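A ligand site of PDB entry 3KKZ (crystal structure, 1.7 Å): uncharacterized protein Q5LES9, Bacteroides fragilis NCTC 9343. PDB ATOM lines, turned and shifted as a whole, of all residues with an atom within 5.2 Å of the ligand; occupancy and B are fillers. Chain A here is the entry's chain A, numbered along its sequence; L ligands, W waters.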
ATOM      1  N   ARG A  25       8.222  -4.878  -3.264  1.00  0.00           N
ATOM      2  CA  ARG A  25       6.898  -5.468  -3.096  1.00  0.00           C
ATOM      3  C   ARG A  25       6.593  -6.338  -4.298  1.00  0.00           C
ATOM      4  O   ARG A  25       7.105  -6.086  -5.401  1.00  0.00           O
ATOM      5  CB  ARG A  25       5.806  -4.379  -3.010  1.00  0.00           C
ATOM      6  CG  ARG A  25       5.849  -3.537  -1.734  1.00  0.00           C
ATOM      7  CD  ARG A  25       5.507  -4.351  -0.503  1.00  0.00           C
ATOM      8  NE  ARG A  25       4.172  -4.945  -0.541  1.00  0.00           N
ATOM      9  CZ  ARG A  25       3.047  -4.329  -0.174  1.00  0.00           C
ATOM     10  NH1 ARG A  25       3.085  -3.066   0.254  1.00  0.00           N
ATOM     11  NH2 ARG A  25       1.890  -4.974  -0.227  1.00  0.00           N
ATOM     12  N   GLN A  26       5.747  -7.349  -4.114  1.00  0.00           N
ATOM     13  CA  GLN A  26       5.391  -8.252  -5.207  1.00  0.00           C
ATOM     14  C   GLN A  26       3.919  -8.171  -5.588  1.00  0.00           C
ATOM     15  O   GLN A  26       3.390  -9.020  -6.308  1.00  0.00           O
ATOM     16  CB  GLN A  26       5.800  -9.693  -4.886  1.00  0.00           C
ATOM     17  CG  GLN A  26       7.309  -9.883  -4.780  1.00  0.00           C
ATOM     18  CD  GLN A  26       7.855  -9.418  -3.446  1.00  0.00           C
ATOM     19  OE1 GLN A  26       7.269  -9.684  -2.398  1.00  0.00           O
ATOM     20  NE2 GLN A  26       8.991  -8.713  -3.474  1.00  0.00           N
ATOM     21  N   GLY A  27       3.264  -7.110  -5.119  1.00  0.00           N
ATOM     22  CA  GLY A  27       1.886  -6.834  -5.505  1.00  0.00           C
ATOM     23  C   GLY A  27       1.538  -5.406  -5.121  1.00  0.00           C
ATOM     24  O   GLY A  27       2.335  -4.722  -4.478  1.00  0.00           O
ATOM     25  N   PRO A  28       0.356  -4.940  -5.535  1.00  0.00           N
ATOM     26  CA  PRO A  28      -0.068  -3.562  -5.258  1.00  0.00           C
ATOM     27  C   PRO A  28      -0.112  -3.275  -3.758  1.00  0.00           C
ATOM     28  O   PRO A  28      -0.502  -4.141  -2.983  1.00  0.00           O
ATOM     29  CB  PRO A  28      -1.489  -3.507  -5.837  1.00  0.00           C
ATOM     30  CG  PRO A  28      -1.462  -4.538  -6.946  1.00  0.00           C
ATOM     31  CD  PRO A  28      -0.567  -5.638  -6.459  1.00  0.00           C
ATOM     32  N   ASP A  52       2.029 -12.910   8.860  1.00  0.00           N
ATOM     33  CA  ASP A  52       1.766 -12.319   7.552  1.00  0.00           C
ATOM     34  C   ASP A  52       1.864 -13.438   6.519  1.00  0.00           C
ATOM     35  O   ASP A  52       2.944 -13.977   6.276  1.00  0.00           O
ATOM     36  CB  ASP A  52       2.784 -11.207   7.274  1.00  0.00           C
ATOM     37  CG  ASP A  52       2.521 -10.483   5.962  1.00  0.00           C
ATOM     38  OD1 ASP A  52       1.464 -10.738   5.340  1.00  0.00           O
ATOM     39  OD2 ASP A  52       3.356  -9.655   5.552  1.00  0.00           O
ATOM     40  N   ILE A  53       0.724 -13.802   5.939  1.00  0.00           N
ATOM     41  CA  ILE A  53       0.609 -14.989   5.083  1.00  0.00           C
ATOM     42  C   ILE A  53       0.790 -14.615   3.612  1.00  0.00           C
ATOM     43  O   ILE A  53       0.184 -13.660   3.135  1.00  0.00           O
ATOM     44  CB  ILE A  53      -0.781 -15.635   5.267  1.00  0.00           C
ATOM     45  CG1 ILE A  53      -1.061 -15.886   6.747  1.00  0.00           C
ATOM     46  CG2 ILE A  53      -0.907 -16.929   4.441  1.00  0.00           C
ATOM     47  CD1 ILE A  53      -0.025 -16.685   7.440  1.00  0.00           C
ATOM     48  N   GLY A  54       1.617 -15.372   2.895  1.00  0.00           N
ATOM     49  CA  GLY A  54       1.987 -14.997   1.534  1.00  0.00           C
ATOM     50  C   GLY A  54       2.772 -13.694   1.521  1.00  0.00           C
ATOM     51  O   GLY A  54       2.520 -12.811   0.694  1.00  0.00           O
ATOM     52  N   CYS A  55       3.740 -13.591   2.430  1.00  0.00           N
ATOM     53  CA  CYS A  55       4.445 -12.335   2.690  1.00  0.00           C
ATOM     54  C   CYS A  55       5.412 -11.891   1.587  1.00  0.00           C
ATOM     55  O   CYS A  55       5.867 -10.748   1.600  1.00  0.00           O
ATOM     56  CB  CYS A  55       5.215 -12.436   4.015  1.00  0.00           C
ATOM     57  SG  CYS A  55       6.468 -13.734   4.018  1.00  0.00           S
ATOM     58  N   GLY A  56       5.731 -12.776   0.658  1.00  0.00           N
ATOM     59  CA  GLY A  56       6.725 -12.432  -0.351  1.00  0.00           C
ATOM     60  C   GLY A  56       8.056 -12.146   0.316  1.00  0.00           C
ATOM     61  O   GLY A  56       8.447 -12.826   1.264  1.00  0.00           O
ATOM     62  N   GLN A  60       5.920  -5.249   3.008  1.00  0.00           N
ATOM     63  CA  GLN A  60       4.849  -4.791   3.908  1.00  0.00           C
ATOM     64  C   GLN A  60       5.075  -5.284   5.337  1.00  0.00           C
ATOM     65  O   GLN A  60       4.681  -4.626   6.299  1.00  0.00           O
ATOM     66  CB  GLN A  60       3.455  -5.201   3.388  1.00  0.00           C
ATOM     67  CG  GLN A  60       3.107  -6.705   3.515  1.00  0.00           C
ATOM     68  CD  GLN A  60       3.936  -7.590   2.593  1.00  0.00           C
ATOM     69  OE1 GLN A  60       4.503  -7.135   1.605  1.00  0.00           O
ATOM     70  NE2 GLN A  60       3.999  -8.880   2.913  1.00  0.00           N
ATOM     71  N   LEU A  75       5.105 -15.826   6.411  1.00  0.00           N
ATOM     72  CA  LEU A  75       5.087 -17.152   5.818  1.00  0.00           C
ATOM     73  C   LEU A  75       4.900 -17.072   4.310  1.00  0.00           C
ATOM     74  O   LEU A  75       4.030 -16.343   3.826  1.00  0.00           O
ATOM     75  CB  LEU A  75       3.971 -18.009   6.452  1.00  0.00           C
ATOM     76  CG  LEU A  75       3.725 -19.402   5.860  1.00  0.00           C
ATOM     77  CD1 LEU A  75       3.231 -20.365   6.940  1.00  0.00           C
ATOM     78  CD2 LEU A  75       2.738 -19.342   4.674  1.00  0.00           C
ATOM     79  N   ASP A  76       5.722 -17.797   3.569  1.00  0.00           N
ATOM     80  CA  ASP A  76       5.558 -17.815   2.113  1.00  0.00           C
ATOM     81  C   ASP A  76       5.947 -19.180   1.572  1.00  0.00           C
ATOM     82  O   ASP A  76       6.766 -19.874   2.162  1.00  0.00           O
ATOM     83  CB  ASP A  76       6.395 -16.724   1.448  1.00  0.00           C
ATOM     84  CG  ASP A  76       5.866 -16.370   0.067  1.00  0.00           C
ATOM     85  OD1 ASP A  76       6.212 -17.053  -0.925  1.00  0.00           O
ATOM     86  OD2 ASP A  76       5.079 -15.400  -0.025  1.00  0.00           O
ATOM     87  N   PHE A  77       5.357 -19.541   0.436  1.00  0.00           N
ATOM     88  CA  PHE A  77       5.642 -20.809  -0.211  1.00  0.00           C
ATOM     89  C   PHE A  77       7.060 -20.847  -0.806  1.00  0.00           C
ATOM     90  O   PHE A  77       7.688 -21.897  -0.861  1.00  0.00           O
ATOM     91  CB  PHE A  77       4.618 -21.066  -1.316  1.00  0.00           C
ATOM     92  CG  PHE A  77       4.822 -22.359  -2.020  1.00  0.00           C
ATOM     93  CD1 PHE A  77       4.383 -23.545  -1.458  1.00  0.00           C
ATOM     94  CD2 PHE A  77       5.470 -22.393  -3.252  1.00  0.00           C
ATOM     95  CE1 PHE A  77       4.585 -24.746  -2.115  1.00  0.00           C
ATOM     96  CE2 PHE A  77       5.678 -23.591  -3.902  1.00  0.00           C
ATOM     97  CZ  PHE A  77       5.231 -24.774  -3.334  1.00  0.00           C
ATOM     98  N   LEU A  78       7.539 -19.697  -1.258  1.00  0.00           N
ATOM     99  CA  LEU A  78       8.820 -19.648  -1.981  1.00  0.00           C
ATOM    100  C   LEU A  78      10.007 -19.396  -1.044  1.00  0.00           C
ATOM    101  O   LEU A  78      10.133 -18.307  -0.488  1.00  0.00           O
ATOM    102  CB  LEU A  78       8.782 -18.568  -3.060  1.00  0.00           C
ATOM    103  CG  LEU A  78       7.893 -18.859  -4.264  1.00  0.00           C
ATOM    104  CD1 LEU A  78       7.964 -17.739  -5.275  1.00  0.00           C
ATOM    105  CD2 LEU A  78       8.298 -20.174  -4.902  1.00  0.00           C
ATOM    106  N   PHE A  81      11.979 -16.225  -1.601  1.00  0.00           N
ATOM    107  CA  PHE A  81      11.408 -15.011  -1.020  1.00  0.00           C
ATOM    108  C   PHE A  81      11.696 -14.941   0.482  1.00  0.00           C
ATOM    109  O   PHE A  81      12.028 -13.870   1.024  1.00  0.00           O
ATOM    110  CB  PHE A  81       9.887 -14.957  -1.240  1.00  0.00           C
ATOM    111  CG  PHE A  81       9.472 -14.520  -2.623  1.00  0.00           C
ATOM    112  CD1 PHE A  81      10.395 -13.990  -3.518  1.00  0.00           C
ATOM    113  CD2 PHE A  81       8.142 -14.611  -3.016  1.00  0.00           C
ATOM    114  CE1 PHE A  81       9.999 -13.577  -4.791  1.00  0.00           C
ATOM    115  CE2 PHE A  81       7.746 -14.197  -4.289  1.00  0.00           C
ATOM    116  CZ  PHE A  81       8.668 -13.685  -5.175  1.00  0.00           C
ATOM    117  N   GLY A 103       6.159 -22.111   4.060  1.00  0.00           N
ATOM    118  CA  GLY A 103       4.955 -22.868   4.308  1.00  0.00           C
ATOM    119  C   GLY A 103       3.893 -22.579   3.277  1.00  0.00           C
ATOM    120  O   GLY A 103       4.070 -21.714   2.414  1.00  0.00           O
ATOM    121  N   SER A 104       2.774 -23.288   3.364  1.00  0.00           N
ATOM    122  CA  SER A 104       1.674 -23.103   2.432  1.00  0.00           C
ATOM    123  C   SER A 104       0.425 -22.643   3.165  1.00  0.00           C
ATOM    124  O   SER A 104       0.098 -23.155   4.241  1.00  0.00           O
ATOM    125  CB  SER A 104       1.392 -24.405   1.686  1.00  0.00           C
ATOM    126  OG  SER A 104       0.374 -24.195   0.724  1.00  0.00           O
ATOM    127  N   MET A 105      -0.299 -21.696   2.571  1.00  0.00           N
ATOM    128  CA  MET A 105      -1.429 -21.088   3.253  1.00  0.00           C
ATOM    129  C   MET A 105      -2.641 -22.014   3.325  1.00  0.00           C
ATOM    130  O   MET A 105      -3.638 -21.688   3.996  1.00  0.00           O
ATOM    131  CB  MET A 105      -1.806 -19.745   2.610  1.00  0.00           C
ATOM    132  CG  MET A 105      -2.336 -19.866   1.203  1.00  0.00           C
ATOM    133  SD  MET A 105      -2.810 -18.121   0.480  1.00  0.00           S
ATOM    134  CE  MET A 105      -1.031 -17.333   0.325  1.00  0.00           C
ATOM    135  N   ASP A 106      -2.579 -23.155   2.642  1.00  0.00           N
ATOM    136  CA  ASP A 106      -3.625 -24.160   2.752  1.00  0.00           C
ATOM    137  C   ASP A 106      -3.305 -25.175   3.852  1.00  0.00           C
ATOM    138  O   ASP A 106      -4.061 -26.129   4.069  1.00  0.00           O
ATOM    139  CB  ASP A 106      -3.896 -24.866   1.412  1.00  0.00           C
ATOM    140  CG  ASP A 106      -2.730 -25.739   0.965  1.00  0.00           C
ATOM    141  OD1 ASP A 106      -1.634 -25.613   1.537  1.00  0.00           O
ATOM    142  OD2 ASP A 106      -2.936 -26.553   0.037  1.00  0.00           O
ATOM    143  N   GLU A 121      -1.369  -9.479   2.297  1.00  0.00           N
ATOM    144  CA  GLU A 121      -1.576  -8.537   1.196  1.00  0.00           C
ATOM    145  C   GLU A 121      -1.349  -9.182  -0.152  1.00  0.00           C
ATOM    146  O   GLU A 121      -0.319  -9.817  -0.389  1.00  0.00           O
ATOM    147  CB  GLU A 121      -0.693  -7.291   1.365  1.00  0.00           C
ATOM    148  CG  GLU A 121      -1.039  -6.475   2.615  1.00  0.00           C
ATOM    149  CD  GLU A 121      -0.445  -5.085   2.598  1.00  0.00           C
ATOM    150  OE1 GLU A 121      -0.422  -4.446   1.521  1.00  0.00           O
ATOM    151  OE2 GLU A 121      -0.006  -4.609   3.680  1.00  0.00           O
ATOM    152  N   GLY A 122      -2.339  -9.045  -1.034  1.00  0.00           N
ATOM    153  CA  GLY A 122      -2.216  -9.537  -2.398  1.00  0.00           C
ATOM    154  C   GLY A 122      -1.830 -11.004  -2.480  1.00  0.00           C
ATOM    155  O   GLY A 122      -1.045 -11.385  -3.346  1.00  0.00           O
ATOM    156  N   ALA A 123      -2.391 -11.831  -1.602  1.00  0.00           N
ATOM    157  CA  ALA A 123      -1.978 -13.234  -1.579  1.00  0.00           C
ATOM    158  C   ALA A 123      -3.094 -14.239  -1.300  1.00  0.00           C
ATOM    159  O   ALA A 123      -2.954 -15.423  -1.643  1.00  0.00           O
ATOM    160  CB  ALA A 123      -0.857 -13.422  -0.564  1.00  0.00           C
ATOM    161  N   TYR A 125      -5.786 -14.702  -2.685  1.00  0.00           N
ATOM    162  CA  TYR A 125      -6.347 -15.224  -3.935  1.00  0.00           C
ATOM    163  C   TYR A 125      -5.769 -16.596  -4.274  1.00  0.00           C
ATOM    164  O   TYR A 125      -6.364 -17.365  -5.041  1.00  0.00           O
ATOM    165  CB  TYR A 125      -6.123 -14.240  -5.087  1.00  0.00           C
ATOM    166  CG  TYR A 125      -4.686 -14.196  -5.564  1.00  0.00           C
ATOM    167  CD1 TYR A 125      -4.200 -15.134  -6.469  1.00  0.00           C
ATOM    168  CD2 TYR A 125      -3.830 -13.215  -5.101  1.00  0.00           C
ATOM    169  CE1 TYR A 125      -2.894 -15.105  -6.900  1.00  0.00           C
ATOM    170  CE2 TYR A 125      -2.509 -13.177  -5.536  1.00  0.00           C
ATOM    171  CZ  TYR A 125      -2.053 -14.117  -6.426  1.00  0.00           C
ATOM    172  OH  TYR A 125      -0.733 -14.073  -6.848  1.00  0.00           O
ATOM    173  N   ASN A 126      -4.597 -16.909  -3.717  1.00  0.00           N
ATOM    174  CA  ASN A 126      -3.982 -18.219  -3.973  1.00  0.00           C
ATOM    175  C   ASN A 126      -4.800 -19.400  -3.460  1.00  0.00           C
ATOM    176  O   ASN A 126      -4.761 -20.490  -4.026  1.00  0.00           O
ATOM    177  CB  ASN A 126      -2.536 -18.270  -3.450  1.00  0.00           C
ATOM    178  CG  ASN A 126      -1.577 -17.475  -4.328  1.00  0.00           C
ATOM    179  OD1 ASN A 126      -1.282 -17.872  -5.448  1.00  0.00           O
ATOM    180  ND2 ASN A 126      -1.102 -16.351  -3.802  1.00  0.00           N
ATOM    181  N   ILE A 127      -5.548 -19.189  -2.375  1.00  0.00           N
ATOM    182  CA  ILE A 127      -6.479 -20.223  -1.938  1.00  0.00           C
ATOM    183  C   ILE A 127      -7.935 -19.823  -2.132  1.00  0.00           C
ATOM    184  O   ILE A 127      -8.825 -20.665  -2.086  1.00  0.00           O
ATOM    185  CB  ILE A 127      -6.254 -20.671  -0.485  1.00  0.00           C
ATOM    186  CG1 ILE A 127      -6.331 -19.482   0.467  1.00  0.00           C
ATOM    187  CG2 ILE A 127      -4.929 -21.404  -0.361  1.00  0.00           C
ATOM    188  CD1 ILE A 127      -6.306 -19.906   1.924  1.00  0.00           C
ATOM    189  N   TYR A 249      -7.856  -3.273  -5.781  1.00  0.00           N
ATOM    190  CA  TYR A 249      -7.643  -4.042  -4.562  1.00  0.00           C
ATOM    191  C   TYR A 249      -8.397  -3.344  -3.449  1.00  0.00           C
ATOM    192  O   TYR A 249      -8.475  -2.121  -3.417  1.00  0.00           O
ATOM    193  CB  TYR A 249      -6.162  -4.042  -4.198  1.00  0.00           C
ATOM    194  CG  TYR A 249      -5.381  -5.285  -4.571  1.00  0.00           C
ATOM    195  CD1 TYR A 249      -5.753  -6.075  -5.645  1.00  0.00           C
ATOM    196  CD2 TYR A 249      -4.243  -5.631  -3.864  1.00  0.00           C
ATOM    197  CE1 TYR A 249      -5.009  -7.202  -5.993  1.00  0.00           C
ATOM    198  CE2 TYR A 249      -3.493  -6.740  -4.198  1.00  0.00           C
ATOM    199  CZ  TYR A 249      -3.886  -7.526  -5.267  1.00  0.00           C
ATOM    200  OH  TYR A 249      -3.164  -8.650  -5.611  1.00  0.00           O
HETATM  201  N1  LIG L   1       2.345 -10.037   0.317  1.00  0.00           N
HETATM  202  C1  LIG L   1       3.360  -9.633  -0.594  1.00  0.00           C
HETATM  203  C2  LIG L   1       3.129  -8.178  -1.092  1.00  0.00           C
HETATM  204  O1  LIG L   1       2.056  -7.700  -0.769  1.00  0.00           O
HETATM  205  O2  LIG L   1       4.136  -7.785  -1.654  1.00  0.00           O
HETATM  206  C3  LIG L   1       3.583 -10.628  -1.833  1.00  0.00           C
HETATM  207  C4  LIG L   1       2.497 -10.370  -2.754  1.00  0.00           C
HETATM  208  S1  LIG L   1       2.417 -11.635  -4.133  1.00  0.00           S
HETATM  209  C5  LIG L   1       1.426 -10.898  -5.469  1.00  0.00           C
HETATM  210  C6  LIG L   1       1.755 -13.281  -3.567  1.00  0.00           C
HETATM  211  C7  LIG L   1       2.617 -14.037  -2.566  1.00  0.00           C
HETATM  212  O3  LIG L   1       1.955 -15.258  -2.227  1.00  0.00           O
HETATM  213  C8  LIG L   1       3.973 -14.468  -3.210  1.00  0.00           C
HETATM  214  O4  LIG L   1       5.019 -14.142  -2.363  1.00  0.00           O
HETATM  215  C9  LIG L   1       3.782 -16.010  -3.450  1.00  0.00           C
HETATM  216  O5  LIG L   1       4.937 -16.769  -3.326  1.00  0.00           O
HETATM  217  C10 LIG L   1       2.849 -16.354  -2.237  1.00  0.00           C
HETATM  218  N2  LIG L   1       2.109 -17.638  -2.334  1.00  0.00           N
HETATM  219  C11 LIG L   1       1.392 -18.259  -3.418  1.00  0.00           C
HETATM  220  N3  LIG L   1       0.803 -19.388  -3.089  1.00  0.00           N
HETATM  221  C12 LIG L   1       1.074 -19.601  -1.745  1.00  0.00           C
HETATM  222  C13 LIG L   1       0.700 -20.650  -0.842  1.00  0.00           C
HETATM  223  N4  LIG L   1      -0.061 -21.712  -1.167  1.00  0.00           N
HETATM  224  N5  LIG L   1       1.140 -20.556   0.460  1.00  0.00           N
HETATM  225  C14 LIG L   1       1.908 -19.475   0.800  1.00  0.00           C
HETATM  226  N6  LIG L   1       2.326 -18.422   0.042  1.00  0.00           N
HETATM  227  C15 LIG L   1       1.871 -18.534  -1.252  1.00  0.00           C
HETATM  228  O   HOH W   1      -1.158 -21.862  -4.223  1.00  0.00           O
HETATM  229  O   HOH W   2       6.918  -7.867  -0.204  1.00  0.00           O
HETATM  230  O   HOH W   3       2.176  -9.810  -8.605  1.00  0.00           O
HETATM  231  O   HOH W   4       1.184 -21.302  -5.645  1.00  0.00           O
HETATM  232  O   HOH W   5       3.471 -13.658  -6.771  1.00  0.00           O
HETATM  233  O   HOH W   6       0.102  -6.965  -2.730  1.00  0.00           O
HETATM  234  O   HOH W   7       1.159 -10.774   2.759  1.00  0.00           O
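Water W6 lies within hydrogen-bond range of an oxygen (O1) of the ligand (2.9 Å) and the backbone carbonyl oxygen of Pro 28 (2.9 Å).
Water W2 lies within hydrogen-bond range of OE1 of Gln 26 (2.9 Å), OE1 of Gln 60 (3.1 Å) and O2 of the ligand (3.1 Å).
The backbone NH of Gly 56 lies within hydrogen-bond range of the side-chain carboxylate of Asp 76, 2.8 Å away.
The guanidinium group (NH2) of Arg 25 lies within salt-bridge range of the side-chain carboxylate (OE1) of Glu 121, at 2.9 Å.
The guanidinium group (NE) of Arg 25 is in hydrogen-bond range of the side-chain amide oxygen (OE1) of Gln 60, 3.1 Å away.
The backbone carbonyl oxygen (O) of Leu 75 lies within hydrogen-bond range of the backbone NH (N) of Gly 54.
The side-chain amide nitrogen of Gln 60 is in hydrogen-bond range of the backbone carbonyl oxygen of Cys 55.
NE2 of Gln 60 is in hydrogen-bond range of OD2 of Asp 52.
The backbone NH (N) of Phe 77 lies close to the backbone carbonyl oxygen (O) of Gly 103, at 3.2 Å.
The backbone NH (N) of Cys 55 sits at hydrogen-bond distance from the backbone carbonyl oxygen (O) of Leu 75.
The side-chain carboxylate (OD2) of Asp 76 lies within hydrogen-bond range of an oxygen (O4) of the ligand.
A nitrogen (N1) of the ligand is in hydrogen-bond range of the backbone carbonyl oxygen of Glu 121 (2.8 Å).
The guanidinium group (NH2) of Arg 25 lies within salt-bridge range of an oxygen (O1) of the ligand (2.8 Å).
The backbone NH (N) of Met 105 is in hydrogen-bond range of a nitrogen (N5) of the ligand, at 2.8 Å.
O of Gly 54 sits at hydrogen-bond distance from N1 of the ligand (2.8 Å).
An oxygen (O2) of the ligand is in hydrogen-bond range of the backbone NH of Gln 26, at 3.0 Å.
N of Gly 56 sits close to O4 of the ligand (3.4 Å).
A nitrogen (N4) of the ligand lies within hydrogen-bond range of the side-chain hydroxyl (OG) of Ser 104, 3.2 Å away.
The side-chain amide oxygen of Asn 126 sits close to a nitrogen (N3) of the ligand (3.5 Å).
The side-chain amide nitrogen (NE2) of Gln 60 lies close to a nitrogen (N1) of the ligand, at 3.3 Å.
A nitrogen (N6) of the ligand lies within hydrogen-bond range of the backbone NH (N) of Phe 77, at 3.3 Å.
S1 of the ligand sits close to O of Gly 122, 3.6 Å away.
Gly 27 touches the ligand (N to O2, 3.6 Å).
Cys 55 touches the ligand (O to C1, 3.5 Å).
Leu 75 touches the ligand.
CD1 of Leu 78 touches O5 of the ligand, at 3.7 Å.
Phe 81 touches the ligand.
Gly 103 touches the ligand.
Ala 123 touches the ligand (CB to O3, 3.7 Å).
Hydrophobic or aromatic side chains that line the ligand: Leu 75, Phe 77, Leu 78, Phe 81, Met 105 and Ala 123.
Of the 26 residues printed, 19 come within 4 Å of the ligand.
Along chain A the residues within 4 Å of the ligand span positions 25 to 126.
The nearest printed residue that does not touch the ligand is Tyr 125 (4.1 Å).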
